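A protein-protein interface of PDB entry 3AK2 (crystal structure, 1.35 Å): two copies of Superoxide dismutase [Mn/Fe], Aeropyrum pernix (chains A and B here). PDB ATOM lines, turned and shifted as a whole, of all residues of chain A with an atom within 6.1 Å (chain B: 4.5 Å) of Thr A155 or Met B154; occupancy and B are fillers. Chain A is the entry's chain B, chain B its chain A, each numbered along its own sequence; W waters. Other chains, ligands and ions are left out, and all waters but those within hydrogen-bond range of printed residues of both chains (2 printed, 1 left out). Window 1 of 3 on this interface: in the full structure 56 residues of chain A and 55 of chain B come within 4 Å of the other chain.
The side-chain hydroxyl of Ser B70 sits at hydrogen-bond distance from the backbone carbonyl oxygen of Leu A153 (2.6 Å). The backbone carbonyl oxygen (O) of Asn B151 is in hydrogen-bond range of the backbone NH (N) of Leu A153. The side-chain hydroxyl (OG) of Ser A70 is in hydrogen-bond range of the backbone carbonyl oxygen (O) of Leu B153. O of Asn A151 sits at hydrogen-bond distance from N of Leu B153 (2.7 Å).
The side-chain hydroxyl (OG) of Ser B70 lies within hydrogen-bond range of the side-chain amide nitrogen (ND2) of Asn B151, 2.9 Å away. The side-chain amide nitrogen (ND2) of Asn A151 sits at hydrogen-bond distance from the side-chain hydroxyl (OG) of Ser A70 (2.9 Å).
Thr B155 touches Ala A74. Met B154 touches Asn A151. O of Asn B151 touches C of Val A152, at 3.8 Å. Met B154 touches Met A154. Thr B155 touches Met A154 (C to CG, 3.8 Å). Ala B74 touches Thr A155. Met B154 touches Thr A155 (CG to C, 3.8 Å). Ala A156 touches Tyr B73. Ala A156 touches Met B154 (N to CG, 3.6 Å). Ala A156 touches Pro B160 (CB to CG, 3.8 Å).
Of the printed residues of chain B, Ser A70 touches Leu B153 (2.6 Å) and Thr B155 (3.4 Å). Printed residues of chain B within 4 Å of Val A152: Asn B151. Of chain B, only Ser B70, Tyr B73, Ala B74 and Met B154 come within 4 Å of Thr A155. Of the printed residues of chain A, Ser B70 touches Leu A153 (2.6 Å) and Thr A155 (3.3 Å). Of the printed residues of chain A, Tyr B73 touches Thr A155, Ala A156 and Leu A158. Of the printed residues of chain A, Ala B74 touches Thr A155 (3.7 Å). Val B147 touches none of the printed residues of chain A. Met B154 touches four residues of chain A. Leu B158 touches none of the printed residues of chain A. The nearest printed residue of chain A that does not touch Thr B155 is Thr A155 (4.3 Å).
Printed residues of chain A that touch a printed residue of chain B: Ser A70, Ala A74, Asn A151, Val A152, Leu A153, Met A154, Thr A155, Ala A156 and Leu A158. Hydrophobic or aromatic side chains of chain A that line the printed part of chain B: Ala A74, Leu A153, Met A154, Ala A156 and Leu A158. Along chain A the printed residues that touch a printed residue of chain B span positions 70 to 158. Among the printed residues, no Asp or Glu carboxylate lies within 4 Å of a Lys or Arg side-chain nitrogen of the other chain.
Ala A74 touches Thr B155, and with the chains exchanged Thr A155 touches Ala B74. Asn A151 touches Val B152, and with the chains exchanged Val A152 touches Asn B151. Asn A151 touches Met B154, and with the chains exchanged Met A154 touches Asn B151. Met A154 touches Thr B155, and with the chains exchanged Thr A155 touches Met B154.
Water W2 bridges the backbone carbonyl oxygen of Leu B158 (2.7 Å) and the backbone NH of Gly A157 (2.9 Å). Water W1 bridges the backbone carbonyl oxygen (O) of Thr B155 (2.7 Å) and the backbone carbonyl oxygen (O) of Thr A155 (2.7 Å).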
ATOM      1  N   SER A  70     -35.409   6.203   1.153  1.00  0.00           N
ATOM      2  CA  SER A  70     -33.968   6.398   1.242  1.00  0.00           C
ATOM      3  C   SER A  70     -33.512   6.527   2.692  1.00  0.00           C
ATOM      4  O   SER A  70     -32.641   5.784   3.140  1.00  0.00           O
ATOM      5  CB  SER A  70     -33.558   7.630   0.436  1.00  0.00           C
ATOM      6  OG  SER A  70     -32.239   8.036   0.765  1.00  0.00           O
ATOM      7  N   ALA A  74     -31.786   3.350   4.597  1.00  0.00           N
ATOM      8  CA  ALA A  74     -30.415   3.625   5.012  1.00  0.00           C
ATOM      9  C   ALA A  74     -30.262   3.456   6.521  1.00  0.00           C
ATOM     10  O   ALA A  74     -29.316   2.815   6.979  1.00  0.00           O
ATOM     11  CB  ALA A  74     -29.993   5.009   4.578  1.00  0.00           C
ATOM     12  N   LEU A 145     -15.087   7.638   5.128  1.00  0.00           N
ATOM     13  CA  LEU A 145     -15.913   8.808   4.847  1.00  0.00           C
ATOM     14  C   LEU A 145     -16.894   9.052   5.983  1.00  0.00           C
ATOM     15  O   LEU A 145     -17.019   8.235   6.902  1.00  0.00           O
ATOM     16  CB  LEU A 145     -16.648   8.670   3.502  1.00  0.00           C
ATOM     17  CG  LEU A 145     -17.803   7.673   3.356  1.00  0.00           C
ATOM     18  CD1 LEU A 145     -18.676   8.038   2.157  1.00  0.00           C
ATOM     19  CD2 LEU A 145     -17.315   6.234   3.237  1.00  0.00           C
ATOM     20  N   HIS A 150     -28.686   9.326   7.561  1.00  0.00           N
ATOM     21  CA  HIS A 150     -28.295   7.983   7.135  1.00  0.00           C
ATOM     22  C   HIS A 150     -27.928   7.907   5.671  1.00  0.00           C
ATOM     23  O   HIS A 150     -27.402   6.894   5.217  1.00  0.00           O
ATOM     24  CB  HIS A 150     -29.429   6.998   7.391  1.00  0.00           C
ATOM     25  CG  HIS A 150     -29.836   6.935   8.819  1.00  0.00           C
ATOM     26  ND1 HIS A 150     -31.145   7.032   9.240  1.00  0.00           N
ATOM     27  CD2 HIS A 150     -29.083   6.829   9.936  1.00  0.00           C
ATOM     28  CE1 HIS A 150     -31.178   6.960  10.560  1.00  0.00           C
ATOM     29  NE2 HIS A 150     -29.941   6.836  11.004  1.00  0.00           N
ATOM     30  N   ASN A 151     -28.202   8.992   4.951  1.00  0.00           N
ATOM     31  CA  ASN A 151     -28.344   8.944   3.503  1.00  0.00           C
ATOM     32  C   ASN A 151     -27.877  10.221   2.831  1.00  0.00           C
ATOM     33  O   ASN A 151     -28.408  10.605   1.791  1.00  0.00           O
ATOM     34  CB  ASN A 151     -29.812   8.660   3.137  1.00  0.00           C
ATOM     35  CG  ASN A 151     -30.754   9.760   3.598  1.00  0.00           C
ATOM     36  OD1 ASN A 151     -30.491  10.462   4.578  1.00  0.00           O
ATOM     37  ND2 ASN A 151     -31.868   9.906   2.898  1.00  0.00           N
ATOM     38  N   VAL A 152     -26.900  10.886   3.438  1.00  0.00           N
ATOM     39  CA  VAL A 152     -26.312  12.084   2.854  1.00  0.00           C
ATOM     40  C   VAL A 152     -24.804  11.887   2.902  1.00  0.00           C
ATOM     41  O   VAL A 152     -24.263  11.533   3.952  1.00  0.00           O
ATOM     42  CB  VAL A 152     -26.743  13.368   3.610  1.00  0.00           C
ATOM     43  CG1 VAL A 152     -26.086  14.597   2.995  1.00  0.00           C
ATOM     44  CG2 VAL A 152     -28.263  13.527   3.586  1.00  0.00           C
ATOM     45  N   LEU A 153     -24.147  12.078   1.758  1.00  0.00           N
ATOM     46  CA  LEU A 153     -22.704  11.825   1.562  1.00  0.00           C
ATOM     47  C   LEU A 153     -22.356  10.372   1.290  1.00  0.00           C
ATOM     48  O   LEU A 153     -21.255  10.079   0.859  1.00  0.00           O
ATOM     49  CB  LEU A 153     -21.818  12.375   2.695  1.00  0.00           C
ATOM     50  CG  LEU A 153     -21.997  13.833   3.119  1.00  0.00           C
ATOM     51  CD1 LEU A 153     -21.043  14.189   4.247  1.00  0.00           C
ATOM     52  CD2 LEU A 153     -21.846  14.799   1.943  1.00  0.00           C
ATOM     53  N   MET A 154     -23.285   9.453   1.532  1.00  0.00           N
ATOM     54  CA  MET A 154     -23.032   8.083   1.121  1.00  0.00           C
ATOM     55  C   MET A 154     -23.024   8.012  -0.408  1.00  0.00           C
ATOM     56  O   MET A 154     -23.744   8.761  -1.086  1.00  0.00           O
ATOM     57  CB  MET A 154     -24.047   7.113   1.727  1.00  0.00           C
ATOM     58  CG  MET A 154     -23.692   5.648   1.473  1.00  0.00           C
ATOM     59  SD  MET A 154     -22.004   5.251   2.013  1.00  0.00           S
ATOM     60  CE  MET A 154     -21.835   3.589   1.366  1.00  0.00           C
ATOM     61  N   THR A 155     -22.179   7.140  -0.946  1.00  0.00           N
ATOM     62  CA  THR A 155     -22.059   6.982  -2.386  1.00  0.00           C
ATOM     63  C   THR A 155     -22.430   5.557  -2.781  1.00  0.00           C
ATOM     64  O   THR A 155     -22.455   4.652  -1.939  1.00  0.00           O
ATOM     65  CB  THR A 155     -20.614   7.243  -2.857  1.00  0.00           C
ATOM     66  OG1 THR A 155     -19.793   6.130  -2.500  1.00  0.00           O
ATOM     67  CG2 THR A 155     -20.032   8.495  -2.215  1.00  0.00           C
ATOM     68  N   ALA A 156     -22.696   5.358  -4.066  1.00  0.00           N
ATOM     69  CA  ALA A 156     -22.771   4.020  -4.627  1.00  0.00           C
ATOM     70  C   ALA A 156     -21.399   3.349  -4.554  1.00  0.00           C
ATOM     71  O   ALA A 156     -20.369   4.014  -4.381  1.00  0.00           O
ATOM     72  CB  ALA A 156     -23.244   4.093  -6.066  1.00  0.00           C
ATOM     73  N   GLY A 157     -21.398   2.025  -4.655  1.00  0.00           N
ATOM     74  CA  GLY A 157     -20.167   1.245  -4.760  1.00  0.00           C
ATOM     75  C   GLY A 157     -19.538   0.876  -3.435  1.00  0.00           C
ATOM     76  O   GLY A 157     -19.436  -0.305  -3.093  1.00  0.00           O
ATOM     77  N   LEU A 158     -19.097   1.890  -2.696  1.00  0.00           N
ATOM     78  CA  LEU A 158     -18.442   1.689  -1.407  1.00  0.00           C
ATOM     79  C   LEU A 158     -19.253   0.780  -0.501  1.00  0.00           C
ATOM     80  O   LEU A 158     -20.435   1.018  -0.274  1.00  0.00           O
ATOM     81  CB  LEU A 158     -18.208   3.030  -0.708  1.00  0.00           C
ATOM     82  CG  LEU A 158     -17.380   4.080  -1.448  1.00  0.00           C
ATOM     83  CD1 LEU A 158     -17.248   5.312  -0.585  1.00  0.00           C
ATOM     84  CD2 LEU A 158     -16.007   3.550  -1.825  1.00  0.00           C
ATOM     85  N   SER B  70     -16.397  12.177  -1.301  1.00  0.00           N
ATOM     86  CA  SER B  70     -17.737  11.645  -1.478  1.00  0.00           C
ATOM     87  C   SER B  70     -18.349  12.101  -2.797  1.00  0.00           C
ATOM     88  O   SER B  70     -18.802  11.284  -3.597  1.00  0.00           O
ATOM     89  CB  SER B  70     -18.626  12.080  -0.317  1.00  0.00           C
ATOM     90  OG  SER B  70     -19.990  11.824  -0.605  1.00  0.00           O
ATOM     91  N   TYR B  73     -15.968  10.915  -5.992  1.00  0.00           N
ATOM     92  CA  TYR B  73     -16.030   9.469  -6.146  1.00  0.00           C
ATOM     93  C   TYR B  73     -17.414   9.054  -6.648  1.00  0.00           C
ATOM     94  O   TYR B  73     -17.536   8.274  -7.599  1.00  0.00           O
ATOM     95  CB  TYR B  73     -15.708   8.737  -4.841  1.00  0.00           C
ATOM     96  CG  TYR B  73     -15.868   7.238  -4.986  1.00  0.00           C
ATOM     97  CD1 TYR B  73     -14.798   6.436  -5.377  1.00  0.00           C
ATOM     98  CD2 TYR B  73     -17.104   6.632  -4.768  1.00  0.00           C
ATOM     99  CE1 TYR B  73     -14.956   5.054  -5.528  1.00  0.00           C
ATOM    100  CE2 TYR B  73     -17.272   5.265  -4.927  1.00  0.00           C
ATOM    101  CZ  TYR B  73     -16.201   4.481  -5.305  1.00  0.00           C
ATOM    102  OH  TYR B  73     -16.395   3.114  -5.438  1.00  0.00           O
ATOM    103  N   ALA B  74     -18.456   9.581  -6.016  1.00  0.00           N
ATOM    104  CA  ALA B  74     -19.810   9.284  -6.446  1.00  0.00           C
ATOM    105  C   ALA B  74     -20.027   9.680  -7.909  1.00  0.00           C
ATOM    106  O   ALA B  74     -20.606   8.918  -8.679  1.00  0.00           O
ATOM    107  CB  ALA B  74     -20.809   9.964  -5.548  1.00  0.00           C
ATOM    108  N   LEU B 145     -34.996   4.583  -6.625  1.00  0.00           N
ATOM    109  CA  LEU B 145     -34.823   5.790  -5.813  1.00  0.00           C
ATOM    110  C   LEU B 145     -34.228   6.932  -6.632  1.00  0.00           C
ATOM    111  O   LEU B 145     -33.808   6.739  -7.781  1.00  0.00           O
ATOM    112  CB  LEU B 145     -33.974   5.512  -4.558  1.00  0.00           C
ATOM    113  CG  LEU B 145     -32.459   5.314  -4.700  1.00  0.00           C
ATOM    114  CD1 LEU B 145     -31.763   5.572  -3.372  1.00  0.00           C
ATOM    115  CD2 LEU B 145     -32.086   3.939  -5.246  1.00  0.00           C
ATOM    116  N   VAL B 147     -31.255  10.092  -6.534  1.00  0.00           N
ATOM    117  CA  VAL B 147     -30.054  10.618  -5.903  1.00  0.00           C
ATOM    118  C   VAL B 147     -29.932  12.086  -6.308  1.00  0.00           C
ATOM    119  O   VAL B 147     -30.089  12.417  -7.486  1.00  0.00           O
ATOM    120  CB  VAL B 147     -28.798   9.813  -6.321  1.00  0.00           C
ATOM    121  CG1 VAL B 147     -27.521  10.470  -5.812  1.00  0.00           C
ATOM    122  CG2 VAL B 147     -28.894   8.367  -5.834  1.00  0.00           C
ATOM    123  N   ASN B 151     -24.408  12.220  -4.438  1.00  0.00           N
ATOM    124  CA  ASN B 151     -24.071  11.667  -3.128  1.00  0.00           C
ATOM    125  C   ASN B 151     -25.028  12.148  -2.054  1.00  0.00           C
ATOM    126  O   ASN B 151     -24.639  12.311  -0.904  1.00  0.00           O
ATOM    127  CB  ASN B 151     -22.634  12.059  -2.755  1.00  0.00           C
ATOM    128  CG  ASN B 151     -22.455  13.565  -2.621  1.00  0.00           C
ATOM    129  OD1 ASN B 151     -23.162  14.355  -3.258  1.00  0.00           O
ATOM    130  ND2 ASN B 151     -21.498  13.967  -1.800  1.00  0.00           N
ATOM    131  N   VAL B 152     -26.275  12.404  -2.436  1.00  0.00           N
ATOM    132  CA  VAL B 152     -27.316  12.782  -1.493  1.00  0.00           C
ATOM    133  C   VAL B 152     -28.514  11.893  -1.801  1.00  0.00           C
ATOM    134  O   VAL B 152     -28.925  11.771  -2.959  1.00  0.00           O
ATOM    135  CB  VAL B 152     -27.681  14.286  -1.607  1.00  0.00           C
ATOM    136  CG1 VAL B 152     -28.803  14.664  -0.632  1.00  0.00           C
ATOM    137  CG2 VAL B 152     -26.445  15.169  -1.369  1.00  0.00           C
ATOM    138  N   LEU B 153     -29.047  11.260  -0.760  1.00  0.00           N
ATOM    139  CA  LEU B 153     -30.137  10.265  -0.840  1.00  0.00           C
ATOM    140  C   LEU B 153     -29.667   8.874  -1.232  1.00  0.00           C
ATOM    141  O   LEU B 153     -30.427   7.914  -1.098  1.00  0.00           O
ATOM    142  CB  LEU B 153     -31.295  10.694  -1.758  1.00  0.00           C
ATOM    143  CG  LEU B 153     -31.928  12.069  -1.537  1.00  0.00           C
ATOM    144  CD1 LEU B 153     -33.054  12.303  -2.537  1.00  0.00           C
ATOM    145  CD2 LEU B 153     -32.425  12.247  -0.112  1.00  0.00           C
ATOM    146  N   MET B 154     -28.438   8.739  -1.722  1.00  0.00           N
ATOM    147  CA  MET B 154     -27.900   7.401  -1.938  1.00  0.00           C
ATOM    148  C   MET B 154     -27.686   6.724  -0.589  1.00  0.00           C
ATOM    149  O   MET B 154     -27.371   7.381   0.406  1.00  0.00           O
ATOM    150  CB  MET B 154     -26.611   7.425  -2.765  1.00  0.00           C
ATOM    151  CG  MET B 154     -26.142   6.033  -3.198  1.00  0.00           C
ATOM    152  SD  MET B 154     -27.450   5.080  -4.011  1.00  0.00           S
ATOM    153  CE  MET B 154     -26.699   3.453  -4.093  1.00  0.00           C
ATOM    154  N   THR B 155     -27.893   5.412  -0.558  1.00  0.00           N
ATOM    155  CA  THR B 155     -27.769   4.641   0.672  1.00  0.00           C
ATOM    156  C   THR B 155     -26.703   3.581   0.485  1.00  0.00           C
ATOM    157  O   THR B 155     -26.332   3.247  -0.643  1.00  0.00           O
ATOM    158  CB  THR B 155     -29.092   3.931   1.044  1.00  0.00           C
ATOM    159  OG1 THR B 155     -29.274   2.788   0.204  1.00  0.00           O
ATOM    160  CG2 THR B 155     -30.287   4.857   0.889  1.00  0.00           C
ATOM    161  N   LEU B 158     -27.688  -0.832  -1.486  1.00  0.00           N
ATOM    162  CA  LEU B 158     -28.304  -0.786  -2.810  1.00  0.00           C
ATOM    163  C   LEU B 158     -27.266  -0.691  -3.916  1.00  0.00           C
ATOM    164  O   LEU B 158     -26.391   0.173  -3.886  1.00  0.00           O
ATOM    165  CB  LEU B 158     -29.272   0.391  -2.908  1.00  0.00           C
ATOM    166  CG  LEU B 158     -30.425   0.433  -1.906  1.00  0.00           C
ATOM    167  CD1 LEU B 158     -31.285   1.656  -2.172  1.00  0.00           C
ATOM    168  CD2 LEU B 158     -31.267  -0.831  -1.951  1.00  0.00           C
ATOM    169  N   PRO B 160     -26.692   0.091  -7.720  1.00  0.00           N
ATOM    170  CA  PRO B 160     -27.279   0.607  -8.959  1.00  0.00           C
ATOM    171  C   PRO B 160     -26.992  -0.307 -10.146  1.00  0.00           C
ATOM    172  O   PRO B 160     -25.837  -0.668 -10.386  1.00  0.00           O
ATOM    173  CB  PRO B 160     -26.587   1.968  -9.145  1.00  0.00           C
ATOM    174  CG  PRO B 160     -26.095   2.338  -7.791  1.00  0.00           C
ATOM    175  CD  PRO B 160     -25.704   1.030  -7.158  1.00  0.00           C
HETATM  176  O   HOH W   1     -23.966   2.432  -1.610  1.00  0.00           O
HETATM  177  O   HOH W   2     -23.806   0.812  -3.725  1.00  0.00           O
